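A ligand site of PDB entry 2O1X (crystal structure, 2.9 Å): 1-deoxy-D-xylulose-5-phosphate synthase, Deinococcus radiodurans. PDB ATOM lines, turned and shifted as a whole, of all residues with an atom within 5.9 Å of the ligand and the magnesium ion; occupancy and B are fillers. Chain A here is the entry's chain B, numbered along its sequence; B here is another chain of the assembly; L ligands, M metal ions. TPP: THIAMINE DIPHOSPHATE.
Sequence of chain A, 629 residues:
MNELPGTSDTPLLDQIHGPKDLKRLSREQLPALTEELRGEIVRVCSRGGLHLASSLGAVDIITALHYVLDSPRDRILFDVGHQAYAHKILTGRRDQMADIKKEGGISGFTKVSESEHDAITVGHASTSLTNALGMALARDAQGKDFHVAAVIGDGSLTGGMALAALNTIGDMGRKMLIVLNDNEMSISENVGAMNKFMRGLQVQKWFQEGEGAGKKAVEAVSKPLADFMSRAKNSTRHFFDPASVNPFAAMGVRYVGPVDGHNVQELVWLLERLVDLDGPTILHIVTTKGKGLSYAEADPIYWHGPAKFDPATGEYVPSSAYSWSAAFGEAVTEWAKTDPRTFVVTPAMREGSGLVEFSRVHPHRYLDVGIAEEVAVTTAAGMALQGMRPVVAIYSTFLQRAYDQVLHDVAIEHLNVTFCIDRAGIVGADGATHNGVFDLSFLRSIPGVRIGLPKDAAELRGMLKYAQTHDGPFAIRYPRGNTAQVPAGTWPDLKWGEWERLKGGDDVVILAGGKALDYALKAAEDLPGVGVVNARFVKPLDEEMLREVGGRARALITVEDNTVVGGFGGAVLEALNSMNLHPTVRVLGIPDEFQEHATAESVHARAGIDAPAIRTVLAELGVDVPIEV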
ATOM      1  N   HIS A  51      35.937 -21.711  13.511  1.00  0.00           N
ATOM      2  CA  HIS A  51      34.473 -21.753  13.600  1.00  0.00           C
ATOM      3  C   HIS A  51      33.947 -20.970  14.795  1.00  0.00           C
ATOM      4  O   HIS A  51      33.663 -21.533  15.846  1.00  0.00           O
ATOM      5  CB  HIS A  51      33.958 -23.198  13.710  1.00  0.00           C
ATOM      6  CG  HIS A  51      34.398 -24.096  12.590  1.00  0.00           C
ATOM      7  ND1 HIS A  51      33.757 -24.150  11.375  1.00  0.00           N
ATOM      8  CD2 HIS A  51      35.415 -24.995  12.522  1.00  0.00           C
ATOM      9  CE1 HIS A  51      34.345 -25.035  10.599  1.00  0.00           C
ATOM     10  NE2 HIS A  51      35.360 -25.569  11.271  1.00  0.00           N
ATOM     11  N   SER A  54      29.155 -21.264  15.237  1.00  0.00           N
ATOM     12  CA  SER A  54      28.607 -22.558  15.651  1.00  0.00           C
ATOM     13  C   SER A  54      28.963 -22.870  17.110  1.00  0.00           C
ATOM     14  O   SER A  54      28.124 -23.372  17.867  1.00  0.00           O
ATOM     15  CB  SER A  54      29.080 -23.669  14.716  1.00  0.00           C
ATOM     16  OG  SER A  54      28.315 -23.716  13.506  1.00  0.00           O
ATOM     17  N   SER A  55      30.191 -22.560  17.500  1.00  0.00           N
ATOM     18  CA  SER A  55      30.667 -22.794  18.850  1.00  0.00           C
ATOM     19  C   SER A  55      30.079 -21.809  19.850  1.00  0.00           C
ATOM     20  O   SER A  55      29.779 -22.179  20.981  1.00  0.00           O
ATOM     21  CB  SER A  55      32.194 -22.715  18.900  1.00  0.00           C
ATOM     22  OG  SER A  55      32.746 -23.841  18.250  1.00  0.00           O
ATOM     23  N   ASP A  79      28.529 -34.098  16.829  1.00  0.00           N
ATOM     24  CA  ASP A  79      28.396 -34.158  15.368  1.00  0.00           C
ATOM     25  C   ASP A  79      29.171 -33.009  14.705  1.00  0.00           C
ATOM     26  O   ASP A  79      29.056 -31.859  15.101  1.00  0.00           O
ATOM     27  CB  ASP A  79      26.908 -34.090  14.983  1.00  0.00           C
ATOM     28  CG  ASP A  79      26.592 -34.778  13.639  1.00  0.00           C
ATOM     29  OD1 ASP A  79      26.686 -34.131  12.566  1.00  0.00           O
ATOM     30  OD2 ASP A  79      26.215 -35.974  13.597  1.00  0.00           O
ATOM     31  N   VAL A  80      29.965 -33.366  13.691  1.00  0.00           N
ATOM     32  CA  VAL A  80      30.916 -32.472  13.005  1.00  0.00           C
ATOM     33  C   VAL A  80      32.040 -32.068  13.942  1.00  0.00           C
ATOM     34  O   VAL A  80      33.205 -32.278  13.635  1.00  0.00           O
ATOM     35  CB  VAL A  80      30.273 -31.235  12.293  1.00  0.00           C
ATOM     36  CG1 VAL A  80      31.302 -30.480  11.482  1.00  0.00           C
ATOM     37  CG2 VAL A  80      29.184 -31.651  11.374  1.00  0.00           C
ATOM     38  N   HIS A  82      32.766 -29.039  15.037  1.00  0.00           N
ATOM     39  CA  HIS A  82      33.128 -27.630  14.840  1.00  0.00           C
ATOM     40  C   HIS A  82      32.508 -26.757  15.925  1.00  0.00           C
ATOM     41  O   HIS A  82      33.052 -25.716  16.270  1.00  0.00           O
ATOM     42  CB  HIS A  82      32.660 -27.163  13.466  1.00  0.00           C
ATOM     43  CG  HIS A  82      31.167 -27.111  13.317  1.00  0.00           C
ATOM     44  ND1 HIS A  82      30.340 -28.135  13.720  1.00  0.00           N
ATOM     45  CD2 HIS A  82      30.352 -26.160  12.804  1.00  0.00           C
ATOM     46  CE1 HIS A  82      29.087 -27.820  13.459  1.00  0.00           C
ATOM     47  NE2 HIS A  82      29.064 -26.620  12.913  1.00  0.00           N
ATOM     48  N   GLN A  83      31.369 -27.191  16.460  1.00  0.00           N
ATOM     49  CA  GLN A  83      30.647 -26.428  17.481  1.00  0.00           C
ATOM     50  C   GLN A  83      31.122 -26.770  18.897  1.00  0.00           C
ATOM     51  O   GLN A  83      30.352 -26.639  19.856  1.00  0.00           O
ATOM     52  CB  GLN A  83      29.112 -26.656  17.337  1.00  0.00           C
ATOM     53  CG  GLN A  83      28.522 -27.950  17.960  1.00  0.00           C
ATOM     54  CD  GLN A  83      29.020 -29.270  17.312  1.00  0.00           C
ATOM     55  OE1 GLN A  83      30.223 -29.449  17.062  1.00  0.00           O
ATOM     56  NE2 GLN A  83      28.096 -30.198  17.070  1.00  0.00           N
ATOM     57  N   GLY A 123      34.113 -34.936  11.530  1.00  0.00           N
ATOM     58  CA  GLY A 123      34.403 -33.820  10.601  1.00  0.00           C
ATOM     59  C   GLY A 123      33.351 -33.810   9.516  1.00  0.00           C
ATOM     60  O   GLY A 123      32.750 -32.777   9.199  1.00  0.00           O
ATOM     61  N   HIS A 124      33.143 -34.993   8.927  1.00  0.00           N
ATOM     62  CA  HIS A 124      31.966 -35.260   8.131  1.00  0.00           C
ATOM     63  C   HIS A 124      30.788 -35.233   9.062  1.00  0.00           C
ATOM     64  O   HIS A 124      30.882 -35.659  10.221  1.00  0.00           O
ATOM     65  CB  HIS A 124      32.109 -36.635   7.495  1.00  0.00           C
ATOM     66  CG  HIS A 124      33.029 -36.669   6.318  1.00  0.00           C
ATOM     67  ND1 HIS A 124      32.966 -37.651   5.348  1.00  0.00           N
ATOM     68  CD2 HIS A 124      34.020 -35.815   5.928  1.00  0.00           C
ATOM     69  CE1 HIS A 124      33.891 -37.409   4.422  1.00  0.00           C
ATOM     70  NE2 HIS A 124      34.543 -36.312   4.758  1.00  0.00           N
ATOM     71  N   ALA A 125      29.663 -34.721   8.570  1.00  0.00           N
ATOM     72  CA  ALA A 125      28.461 -34.601   9.384  1.00  0.00           C
ATOM     73  C   ALA A 125      27.627 -35.885   9.499  1.00  0.00           C
ATOM     74  O   ALA A 125      27.720 -36.811   8.676  1.00  0.00           O
ATOM     75  CB  ALA A 125      27.596 -33.477   8.851  1.00  0.00           C
ATOM     76  N   ILE A 152      23.668 -33.059  18.152  1.00  0.00           N
ATOM     77  CA  ILE A 152      23.544 -33.001  16.703  1.00  0.00           C
ATOM     78  C   ILE A 152      22.798 -31.759  16.246  1.00  0.00           C
ATOM     79  O   ILE A 152      21.698 -31.461  16.702  1.00  0.00           O
ATOM     80  CB  ILE A 152      22.890 -34.297  16.140  1.00  0.00           C
ATOM     81  CG1 ILE A 152      22.889 -34.248  14.612  1.00  0.00           C
ATOM     82  CG2 ILE A 152      21.479 -34.516  16.726  1.00  0.00           C
ATOM     83  CD1 ILE A 152      22.521 -35.543  13.925  1.00  0.00           C
ATOM     84  N   GLY A 153      23.404 -31.013  15.338  1.00  0.00           N
ATOM     85  CA  GLY A 153      22.745 -29.848  14.804  1.00  0.00           C
ATOM     86  C   GLY A 153      21.655 -30.145  13.791  1.00  0.00           C
ATOM     87  O   GLY A 153      21.638 -31.175  13.132  1.00  0.00           O
ATOM     88  N   ASP A 154      20.756 -29.182  13.668  1.00  0.00           N
ATOM     89  CA  ASP A 154      19.666 -29.267  12.718  1.00  0.00           C
ATOM     90  C   ASP A 154      20.142 -29.545  11.299  1.00  0.00           C
ATOM     91  O   ASP A 154      19.428 -30.208  10.549  1.00  0.00           O
ATOM     92  CB  ASP A 154      18.843 -27.986  12.764  1.00  0.00           C
ATOM     93  CG  ASP A 154      19.668 -26.748  12.512  1.00  0.00           C
ATOM     94  OD1 ASP A 154      19.274 -25.977  11.619  1.00  0.00           O
ATOM     95  OD2 ASP A 154      20.727 -26.467  13.144  1.00  0.00           O
ATOM     96  N   GLY A 155      21.313 -29.038  10.923  1.00  0.00           N
ATOM     97  CA  GLY A 155      21.829 -29.233   9.570  1.00  0.00           C
ATOM     98  C   GLY A 155      22.208 -30.697   9.357  1.00  0.00           C
ATOM     99  O   GLY A 155      21.838 -31.331   8.361  1.00  0.00           O
ATOM    100  N   SER A 156      22.943 -31.221  10.318  1.00  0.00           N
ATOM    101  CA  SER A 156      23.336 -32.607  10.311  1.00  0.00           C
ATOM    102  C   SER A 156      22.152 -33.562  10.364  1.00  0.00           C
ATOM    103  O   SER A 156      22.242 -34.684   9.871  1.00  0.00           O
ATOM    104  CB  SER A 156      24.270 -32.888  11.466  1.00  0.00           C
ATOM    105  OG  SER A 156      25.336 -31.959  11.456  1.00  0.00           O
ATOM    106  N   LEU A 157      21.041 -33.134  10.944  1.00  0.00           N
ATOM    107  CA  LEU A 157      19.909 -34.033  11.066  1.00  0.00           C
ATOM    108  C   LEU A 157      19.377 -34.398   9.666  1.00  0.00           C
ATOM    109  O   LEU A 157      18.710 -35.410   9.512  1.00  0.00           O
ATOM    110  CB  LEU A 157      18.804 -33.465  11.992  1.00  0.00           C
ATOM    111  CG  LEU A 157      17.669 -34.396  12.477  1.00  0.00           C
ATOM    112  CD1 LEU A 157      18.206 -35.557  13.320  1.00  0.00           C
ATOM    113  CD2 LEU A 157      16.604 -33.635  13.232  1.00  0.00           C
ATOM    114  N   ASN A 181      20.512 -29.685  18.444  1.00  0.00           N
ATOM    115  CA  ASN A 181      20.954 -28.304  18.525  1.00  0.00           C
ATOM    116  C   ASN A 181      20.452 -27.534  17.308  1.00  0.00           C
ATOM    117  O   ASN A 181      21.081 -27.547  16.246  1.00  0.00           O
ATOM    118  CB  ASN A 181      22.472 -28.272  18.609  1.00  0.00           C
ATOM    119  CG  ASN A 181      23.044 -26.871  18.761  1.00  0.00           C
ATOM    120  OD1 ASN A 181      22.302 -25.891  18.895  1.00  0.00           O
ATOM    121  ND2 ASN A 181      24.365 -26.770  18.753  1.00  0.00           N
ATOM    122  N   ASP A 182      19.308 -26.865  17.488  1.00  0.00           N
ATOM    123  CA  ASP A 182      18.571 -26.287  16.378  1.00  0.00           C
ATOM    124  C   ASP A 182      18.778 -24.769  16.274  1.00  0.00           C
ATOM    125  O   ASP A 182      18.406 -24.008  17.162  1.00  0.00           O
ATOM    126  CB  ASP A 182      17.092 -26.675  16.494  1.00  0.00           C
ATOM    127  CG  ASP A 182      16.232 -26.180  15.344  1.00  0.00           C
ATOM    128  OD1 ASP A 182      14.993 -26.331  15.429  1.00  0.00           O
ATOM    129  OD2 ASP A 182      16.669 -25.630  14.312  1.00  0.00           O
ATOM    130  N   ASN A 183      19.383 -24.373  15.152  1.00  0.00           N
ATOM    131  CA  ASN A 183      19.747 -22.992  14.814  1.00  0.00           C
ATOM    132  C   ASN A 183      18.872 -22.386  13.728  1.00  0.00           C
ATOM    133  O   ASN A 183      18.868 -21.155  13.553  1.00  0.00           O
ATOM    134  CB  ASN A 183      21.128 -23.017  14.178  1.00  0.00           C
ATOM    135  CG  ASN A 183      22.237 -22.801  15.159  1.00  0.00           C
ATOM    136  OD1 ASN A 183      22.048 -22.184  16.229  1.00  0.00           O
ATOM    137  ND2 ASN A 183      23.424 -23.277  14.795  1.00  0.00           N
ATOM    138  N   GLU A 184      18.160 -23.258  12.990  1.00  0.00           N
ATOM    139  CA  GLU A 184      17.697 -23.024  11.599  1.00  0.00           C
ATOM    140  C   GLU A 184      18.796 -22.591  10.620  1.00  0.00           C
ATOM    141  O   GLU A 184      18.521 -22.024   9.547  1.00  0.00           O
ATOM    142  CB  GLU A 184      16.452 -22.150  11.475  1.00  0.00           C
ATOM    143  CG  GLU A 184      15.865 -21.594  12.751  1.00  0.00           C
ATOM    144  CD  GLU A 184      14.405 -21.288  12.572  1.00  0.00           C
ATOM    145  OE1 GLU A 184      13.605 -21.742  13.409  1.00  0.00           O
ATOM    146  OE2 GLU A 184      14.046 -20.632  11.570  1.00  0.00           O
ATOM    147  N   MET A 185      20.038 -22.892  11.004  1.00  0.00           N
ATOM    148  CA  MET A 185      21.218 -22.600  10.205  1.00  0.00           C
ATOM    149  C   MET A 185      22.016 -23.873   9.950  1.00  0.00           C
ATOM    150  O   MET A 185      22.224 -24.710  10.857  1.00  0.00           O
ATOM    151  CB  MET A 185      22.099 -21.554  10.918  1.00  0.00           C
ATOM    152  CG  MET A 185      21.462 -20.193  11.033  1.00  0.00           C
ATOM    153  SD  MET A 185      21.438 -19.367   9.434  1.00  0.00           S
ATOM    154  CE  MET A 185      20.217 -18.098   9.755  1.00  0.00           C
ATOM    155  N   SER A 186      22.425 -24.039   8.697  1.00  0.00           N
ATOM    156  CA  SER A 186      23.458 -25.003   8.337  1.00  0.00           C
ATOM    157  C   SER A 186      24.766 -24.182   8.269  1.00  0.00           C
ATOM    158  O   SER A 186      25.199 -23.662   9.284  1.00  0.00           O
ATOM    159  CB  SER A 186      23.093 -25.709   7.022  1.00  0.00           C
ATOM    160  OG  SER A 186      23.714 -26.996   6.947  1.00  0.00           O
ATOM    161  N   ILE A 187      25.399 -24.076   7.099  1.00  0.00           N
ATOM    162  CA  ILE A 187      26.308 -22.965   6.887  1.00  0.00           C
ATOM    163  C   ILE A 187      25.439 -21.885   6.240  1.00  0.00           C
ATOM    164  O   ILE A 187      25.159 -20.845   6.850  1.00  0.00           O
ATOM    165  CB  ILE A 187      27.555 -23.325   6.002  1.00  0.00           C
ATOM    166  CG1 ILE A 187      28.329 -24.507   6.587  1.00  0.00           C
ATOM    167  CG2 ILE A 187      28.467 -22.114   5.829  1.00  0.00           C
ATOM    168  CD1 ILE A 187      29.772 -24.583   6.134  1.00  0.00           C
ATOM    169  N   ASN A 190      19.737 -23.704   6.910  1.00  0.00           N
ATOM    170  CA  ASN A 190      19.143 -25.024   6.670  1.00  0.00           C
ATOM    171  C   ASN A 190      18.012 -25.099   5.640  1.00  0.00           C
ATOM    172  O   ASN A 190      17.389 -24.093   5.301  1.00  0.00           O
ATOM    173  CB  ASN A 190      18.660 -25.600   8.007  1.00  0.00           C
ATOM    174  CG  ASN A 190      18.805 -27.117   8.089  1.00  0.00           C
ATOM    175  OD1 ASN A 190      18.428 -27.717   9.095  1.00  0.00           O
ATOM    176  ND2 ASN A 190      19.359 -27.735   7.054  1.00  0.00           N
ATOM    177  N   LYS A 289      22.623 -19.100  16.274  1.00  0.00           N
ATOM    178  CA  LYS A 289      24.006 -19.183  15.846  1.00  0.00           C
ATOM    179  C   LYS A 289      24.747 -17.871  16.147  1.00  0.00           C
ATOM    180  O   LYS A 289      24.270 -16.774  15.833  1.00  0.00           O
ATOM    181  CB  LYS A 289      24.102 -19.534  14.349  1.00  0.00           C
ATOM    182  CG  LYS A 289      25.034 -20.713  14.064  1.00  0.00           C
ATOM    183  CD  LYS A 289      26.094 -20.327  13.080  1.00  0.00           C
ATOM    184  CE  LYS A 289      26.663 -21.523  12.330  1.00  0.00           C
ATOM    185  NZ  LYS A 289      26.063 -21.640  10.964  1.00  0.00           N
ATOM    186  N   HIS A 304      30.336 -18.145  10.547  1.00  0.00           N
ATOM    187  CA  HIS A 304      30.656 -19.567  10.649  1.00  0.00           C
ATOM    188  C   HIS A 304      32.186 -19.760  10.585  1.00  0.00           C
ATOM    189  O   HIS A 304      32.768 -20.490  11.398  1.00  0.00           O
ATOM    190  CB  HIS A 304      29.955 -20.315   9.509  1.00  0.00           C
ATOM    191  CG  HIS A 304      30.057 -21.808   9.607  1.00  0.00           C
ATOM    192  ND1 HIS A 304      31.021 -22.528   8.946  1.00  0.00           N
ATOM    193  CD2 HIS A 304      29.290 -22.712  10.254  1.00  0.00           C
ATOM    194  CE1 HIS A 304      30.868 -23.819   9.204  1.00  0.00           C
ATOM    195  NE2 HIS A 304      29.812 -23.954   9.994  1.00  0.00           N
ATOM    196  N   PRO A 347      25.211 -30.135  -2.162  1.00  0.00           N
ATOM    197  CA  PRO A 347      24.867 -30.699  -0.885  1.00  0.00           C
ATOM    198  C   PRO A 347      25.344 -29.767   0.247  1.00  0.00           C
ATOM    199  O   PRO A 347      26.447 -29.966   0.789  1.00  0.00           O
ATOM    200  CB  PRO A 347      25.597 -32.045  -0.895  1.00  0.00           C
ATOM    201  CG  PRO A 347      26.795 -31.809  -1.712  1.00  0.00           C
ATOM    202  CD  PRO A 347      26.509 -30.627  -2.631  1.00  0.00           C
ATOM    203  N   ALA A 348      24.514 -28.771   0.554  1.00  0.00           N
ATOM    204  CA  ALA A 348      24.691 -27.828   1.687  1.00  0.00           C
ATOM    205  C   ALA A 348      25.823 -26.800   1.573  1.00  0.00           C
ATOM    206  O   ALA A 348      26.151 -26.149   2.557  1.00  0.00           O
ATOM    207  CB  ALA A 348      24.801 -28.603   3.009  1.00  0.00           C
ATOM    208  N   MET A 349      26.400 -26.620   0.395  1.00  0.00           N
ATOM    209  CA  MET A 349      27.631 -25.852   0.280  1.00  0.00           C
ATOM    210  C   MET A 349      27.556 -24.709  -0.766  1.00  0.00           C
ATOM    211  O   MET A 349      28.462 -24.543  -1.588  1.00  0.00           O
ATOM    212  CB  MET A 349      28.796 -26.802  -0.039  1.00  0.00           C
ATOM    213  CG  MET A 349      29.187 -27.777   1.080  1.00  0.00           C
ATOM    214  SD  MET A 349      30.400 -27.103   2.250  1.00  0.00           S
ATOM    215  CE  MET A 349      29.228 -26.623   3.509  1.00  0.00           C
ATOM    216  N   ILE A 371      22.715 -31.586   3.982  1.00  0.00           N
ATOM    217  CA  ILE A 371      23.977 -32.323   4.128  1.00  0.00           C
ATOM    218  C   ILE A 371      23.782 -33.780   3.665  1.00  0.00           C
ATOM    219  O   ILE A 371      23.988 -34.739   4.421  1.00  0.00           O
ATOM    220  CB  ILE A 371      24.519 -32.235   5.580  1.00  0.00           C
ATOM    221  CG1 ILE A 371      24.376 -30.811   6.113  1.00  0.00           C
ATOM    222  CG2 ILE A 371      25.974 -32.657   5.599  1.00  0.00           C
ATOM    223  CD1 ILE A 371      24.997 -30.558   7.487  1.00  0.00           C
ATOM    224  N   GLU A 373      24.763 -35.644   0.416  1.00  0.00           N
ATOM    225  CA  GLU A 373      25.485 -35.883  -0.819  1.00  0.00           C
ATOM    226  C   GLU A 373      24.848 -36.997  -1.626  1.00  0.00           C
ATOM    227  O   GLU A 373      24.752 -36.894  -2.858  1.00  0.00           O
ATOM    228  CB  GLU A 373      26.941 -36.192  -0.531  1.00  0.00           C
ATOM    229  CG  GLU A 373      27.736 -34.995  -0.013  1.00  0.00           C
ATOM    230  CD  GLU A 373      27.531 -34.672   1.463  1.00  0.00           C
ATOM    231  OE1 GLU A 373      26.690 -35.305   2.135  1.00  0.00           O
ATOM    232  OE2 GLU A 373      28.222 -33.757   1.964  1.00  0.00           O
ATOM    233  N   PHE A 398      33.435 -34.758   0.472  1.00  0.00           N
ATOM    234  CA  PHE A 398      32.044 -35.050   0.647  1.00  0.00           C
ATOM    235  C   PHE A 398      31.531 -35.999  -0.459  1.00  0.00           C
ATOM    236  O   PHE A 398      30.659 -36.858  -0.194  1.00  0.00           O
ATOM    237  CB  PHE A 398      31.251 -33.777   0.889  1.00  0.00           C
ATOM    238  CG  PHE A 398      31.798 -32.951   2.041  1.00  0.00           C
ATOM    239  CD1 PHE A 398      32.200 -33.579   3.221  1.00  0.00           C
ATOM    240  CD2 PHE A 398      31.939 -31.565   1.922  1.00  0.00           C
ATOM    241  CE1 PHE A 398      32.729 -32.834   4.277  1.00  0.00           C
ATOM    242  CE2 PHE A 398      32.459 -30.821   2.968  1.00  0.00           C
ATOM    243  CZ  PHE A 398      32.863 -31.454   4.156  1.00  0.00           C
ATOM    244  N   ARG A 401      30.979 -39.715   0.310  1.00  0.00           N
ATOM    245  CA  ARG A 401      29.638 -40.092   0.723  1.00  0.00           C
ATOM    246  C   ARG A 401      28.704 -40.563  -0.414  1.00  0.00           C
ATOM    247  O   ARG A 401      27.684 -41.210  -0.163  1.00  0.00           O
ATOM    248  CB  ARG A 401      28.963 -38.934   1.468  1.00  0.00           C
ATOM    249  CG  ARG A 401      29.358 -38.786   2.880  1.00  0.00           C
ATOM    250  CD  ARG A 401      28.583 -39.624   3.830  1.00  0.00           C
ATOM    251  NE  ARG A 401      29.199 -39.548   5.141  1.00  0.00           N
ATOM    252  CZ  ARG A 401      28.835 -38.697   6.085  1.00  0.00           C
ATOM    253  NH1 ARG A 401      27.813 -37.864   5.891  1.00  0.00           N
ATOM    254  NH2 ARG A 401      29.482 -38.673   7.242  1.00  0.00           N
ATOM    255  N   HIS A 434      39.065 -34.099   6.056  1.00  0.00           N
ATOM    256  CA  HIS A 434      38.738 -33.268   4.874  1.00  0.00           C
ATOM    257  C   HIS A 434      39.690 -33.310   3.707  1.00  0.00           C
ATOM    258  O   HIS A 434      39.378 -32.771   2.651  1.00  0.00           O
ATOM    259  CB  HIS A 434      38.585 -31.808   5.285  1.00  0.00           C
ATOM    260  CG  HIS A 434      37.362 -31.546   6.087  1.00  0.00           C
ATOM    261  ND1 HIS A 434      37.127 -32.156   7.301  1.00  0.00           N
ATOM    262  CD2 HIS A 434      36.298 -30.756   5.841  1.00  0.00           C
ATOM    263  CE1 HIS A 434      35.979 -31.730   7.781  1.00  0.00           C
ATOM    264  NE2 HIS A 434      35.457 -30.882   6.914  1.00  0.00           N
ATOM    265  N   ASP B 404      32.402 -44.070   2.397  1.00  0.00           N
ATOM    266  CA  ASP B 404      32.735 -42.983   3.329  1.00  0.00           C
ATOM    267  C   ASP B 404      32.731 -43.349   4.814  1.00  0.00           C
ATOM    268  O   ASP B 404      33.533 -42.789   5.605  1.00  0.00           O
ATOM    269  CB  ASP B 404      31.906 -41.721   3.143  1.00  0.00           C
ATOM    270  CG  ASP B 404      32.519 -40.576   3.891  1.00  0.00           C
ATOM    271  OD1 ASP B 404      31.935 -40.063   4.893  1.00  0.00           O
ATOM    272  OD2 ASP B 404      33.670 -40.187   3.581  1.00  0.00           O
HETATM  273  N1' TPP L   1      29.022 -32.641   4.271  1.00  0.00           N
HETATM  274  C2' TPP L   1      29.441 -33.489   5.230  1.00  0.00           C
HETATM  275  CM2 TPP L   1      29.244 -35.007   5.085  1.00  0.00           C
HETATM  276  N3' TPP L   1      30.050 -33.023   6.315  1.00  0.00           N
HETATM  277  C4' TPP L   1      30.257 -31.713   6.483  1.00  0.00           C
HETATM  278  N4' TPP L   1      30.883 -31.298   7.580  1.00  0.00           N
HETATM  279  C5' TPP L   1      29.822 -30.816   5.512  1.00  0.00           C
HETATM  280  C6' TPP L   1      29.199 -31.342   4.392  1.00  0.00           C
HETATM  281  C7' TPP L   1      29.996 -29.298   5.553  1.00  0.00           C
HETATM  282  N3  TPP L   1      29.618 -28.695   6.845  1.00  0.00           N
HETATM  283  C2  TPP L   1      30.540 -28.498   7.833  1.00  0.00           C
HETATM  284  S1  TPP L   1      29.674 -27.769   9.171  1.00  0.00           S
HETATM  285  C5  TPP L   1      28.171 -27.715   8.351  1.00  0.00           C
HETATM  286  C4  TPP L   1      28.355 -28.279   7.094  1.00  0.00           C
HETATM  287  CM4 TPP L   1      27.228 -28.406   6.079  1.00  0.00           C
HETATM  288  C6  TPP L   1      26.904 -27.155   8.965  1.00  0.00           C
HETATM  289  C7  TPP L   1      26.315 -28.117   9.987  1.00  0.00           C
HETATM  290  O7  TPP L   1      24.999 -27.660  10.316  1.00  0.00           O
HETATM  291  PA  TPP L   1      24.545 -27.738  11.818  1.00  0.00           P
HETATM  292  O1A TPP L   1      24.428 -29.128  12.309  1.00  0.00           O
HETATM  293  O2A TPP L   1      23.189 -26.865  11.985  1.00  0.00           O
HETATM  294  O3A TPP L   1      25.729 -26.957  12.586  1.00  0.00           O
HETATM  295  PB  TPP L   1      25.543 -25.549  13.380  1.00  0.00           P
HETATM  296  O1B TPP L   1      26.519 -25.446  14.487  1.00  0.00           O
HETATM  297  O2B TPP L   1      25.670 -24.330  12.371  1.00  0.00           O
HETATM  298  O3B TPP L   1      23.975 -25.517  13.905  1.00  0.00           O
HETATM  299 MG    MG M   1      22.367 -25.349  13.105  1.00  0.00          MG
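ND2 of Asn 183 lies within hydrogen-bond range of O2B of the ligand. An oxygen (O1B) of the ligand is in hydrogen-bond range of the side-chain hydroxyl (OG) of Ser 54, 2.7 Å away. The side-chain carboxylate (OE2) of Glu 373 lies within hydrogen-bond range of a nitrogen (N1') of the ligand (2.7 Å). N3' of the ligand lies within hydrogen-bond range of N of Ala 125, 2.8 Å away. O of Gly 123 sits at hydrogen-bond distance from N4' of the ligand (2.9 Å). O2B of the ligand lies within salt-bridge range of NZ of Lys 289 (3.1 Å). N of Gly 155 lies within hydrogen-bond range of O1A of the ligand (3.4 Å). N of Ser 156 sits at hydrogen-bond distance from O1A of the ligand. OG of Ser 156 lies within hydrogen-bond range of O1A of the ligand. NE2 of His 82 sits at hydrogen-bond distance from O1B of the ligand (3.2 Å).
The backbone NH (N) of Asn 183 sits close to the side-chain carboxylate (OD2) of Asp 154, at 3.2 Å. The backbone carbonyl oxygen of Asn 181 lies within hydrogen-bond range of the backbone NH of Asp 154 (3.1 Å). The side-chain carboxylate of Asp 154 sits at hydrogen-bond distance from the backbone NH of Glu 184, at 3.2 Å. The backbone NH (N) of Lys 289 lies within hydrogen-bond range of the side-chain amide oxygen (OD1) of Asn 183 (3.1 Å). The backbone carbonyl oxygen (O) of Ser 186 lies within hydrogen-bond range of the side-chain amino group (NZ) of Lys 289 (2.8 Å). The side-chain hydroxyl of Ser 156 is in hydrogen-bond range of the side-chain carboxylate of Asp 79, at 2.8 Å. The side-chain hydroxyl of Ser 55 lies within hydrogen-bond range of the backbone carbonyl oxygen of His 82, at 2.7 Å. NE of Arg 401 is in salt-bridge range of OD1 of Asp 404 of chain B, 2.8 Å away.
An oxygen (O2B) of the ligand lies close to the backbone carbonyl oxygen (O) of Ser 186, at 3.2 Å. Merely in contact with the ligand: Val 80 (3.9 Å), His 124 (3.5 Å), Gly 153 (3.1 Å), Ile 187 (3.7 Å), His 304 (3.9 Å), Ala 348 (3.9 Å), Met 349 (3.5 Å), Ile 371 (3.3 Å), Phe 398 (3.4 Å) and Arg 401 (3.3 Å). Hydrophobic or aromatic side chains that line the ligand: Val 80, His 82, Ala 125, Ile 187, Ala 348, Met 349, Ile 371 and Phe 398. The nearest printed residue that does not touch the ligand is Gln 83 (4.04 Å).
Merely in contact with the magnesium ion: Asn 183 (2.9 Å). Three residues have an atom within 4 Å of the magnesium ion: Asp 154, Asn 183 and Met 185.
An oxygen (O3B) of the ligand is bound to the magnesium ion. The magnesium ion is bound by the side-chain carboxylate (OD2) of Asp 154, 2.0 Å away. The magnesium ion is bound by O2A of the ligand (2.1 Å). O of Met 185 is bound to the magnesium ion, at 2.3 Å. The magnesium ion has four donor atoms within binding distance.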
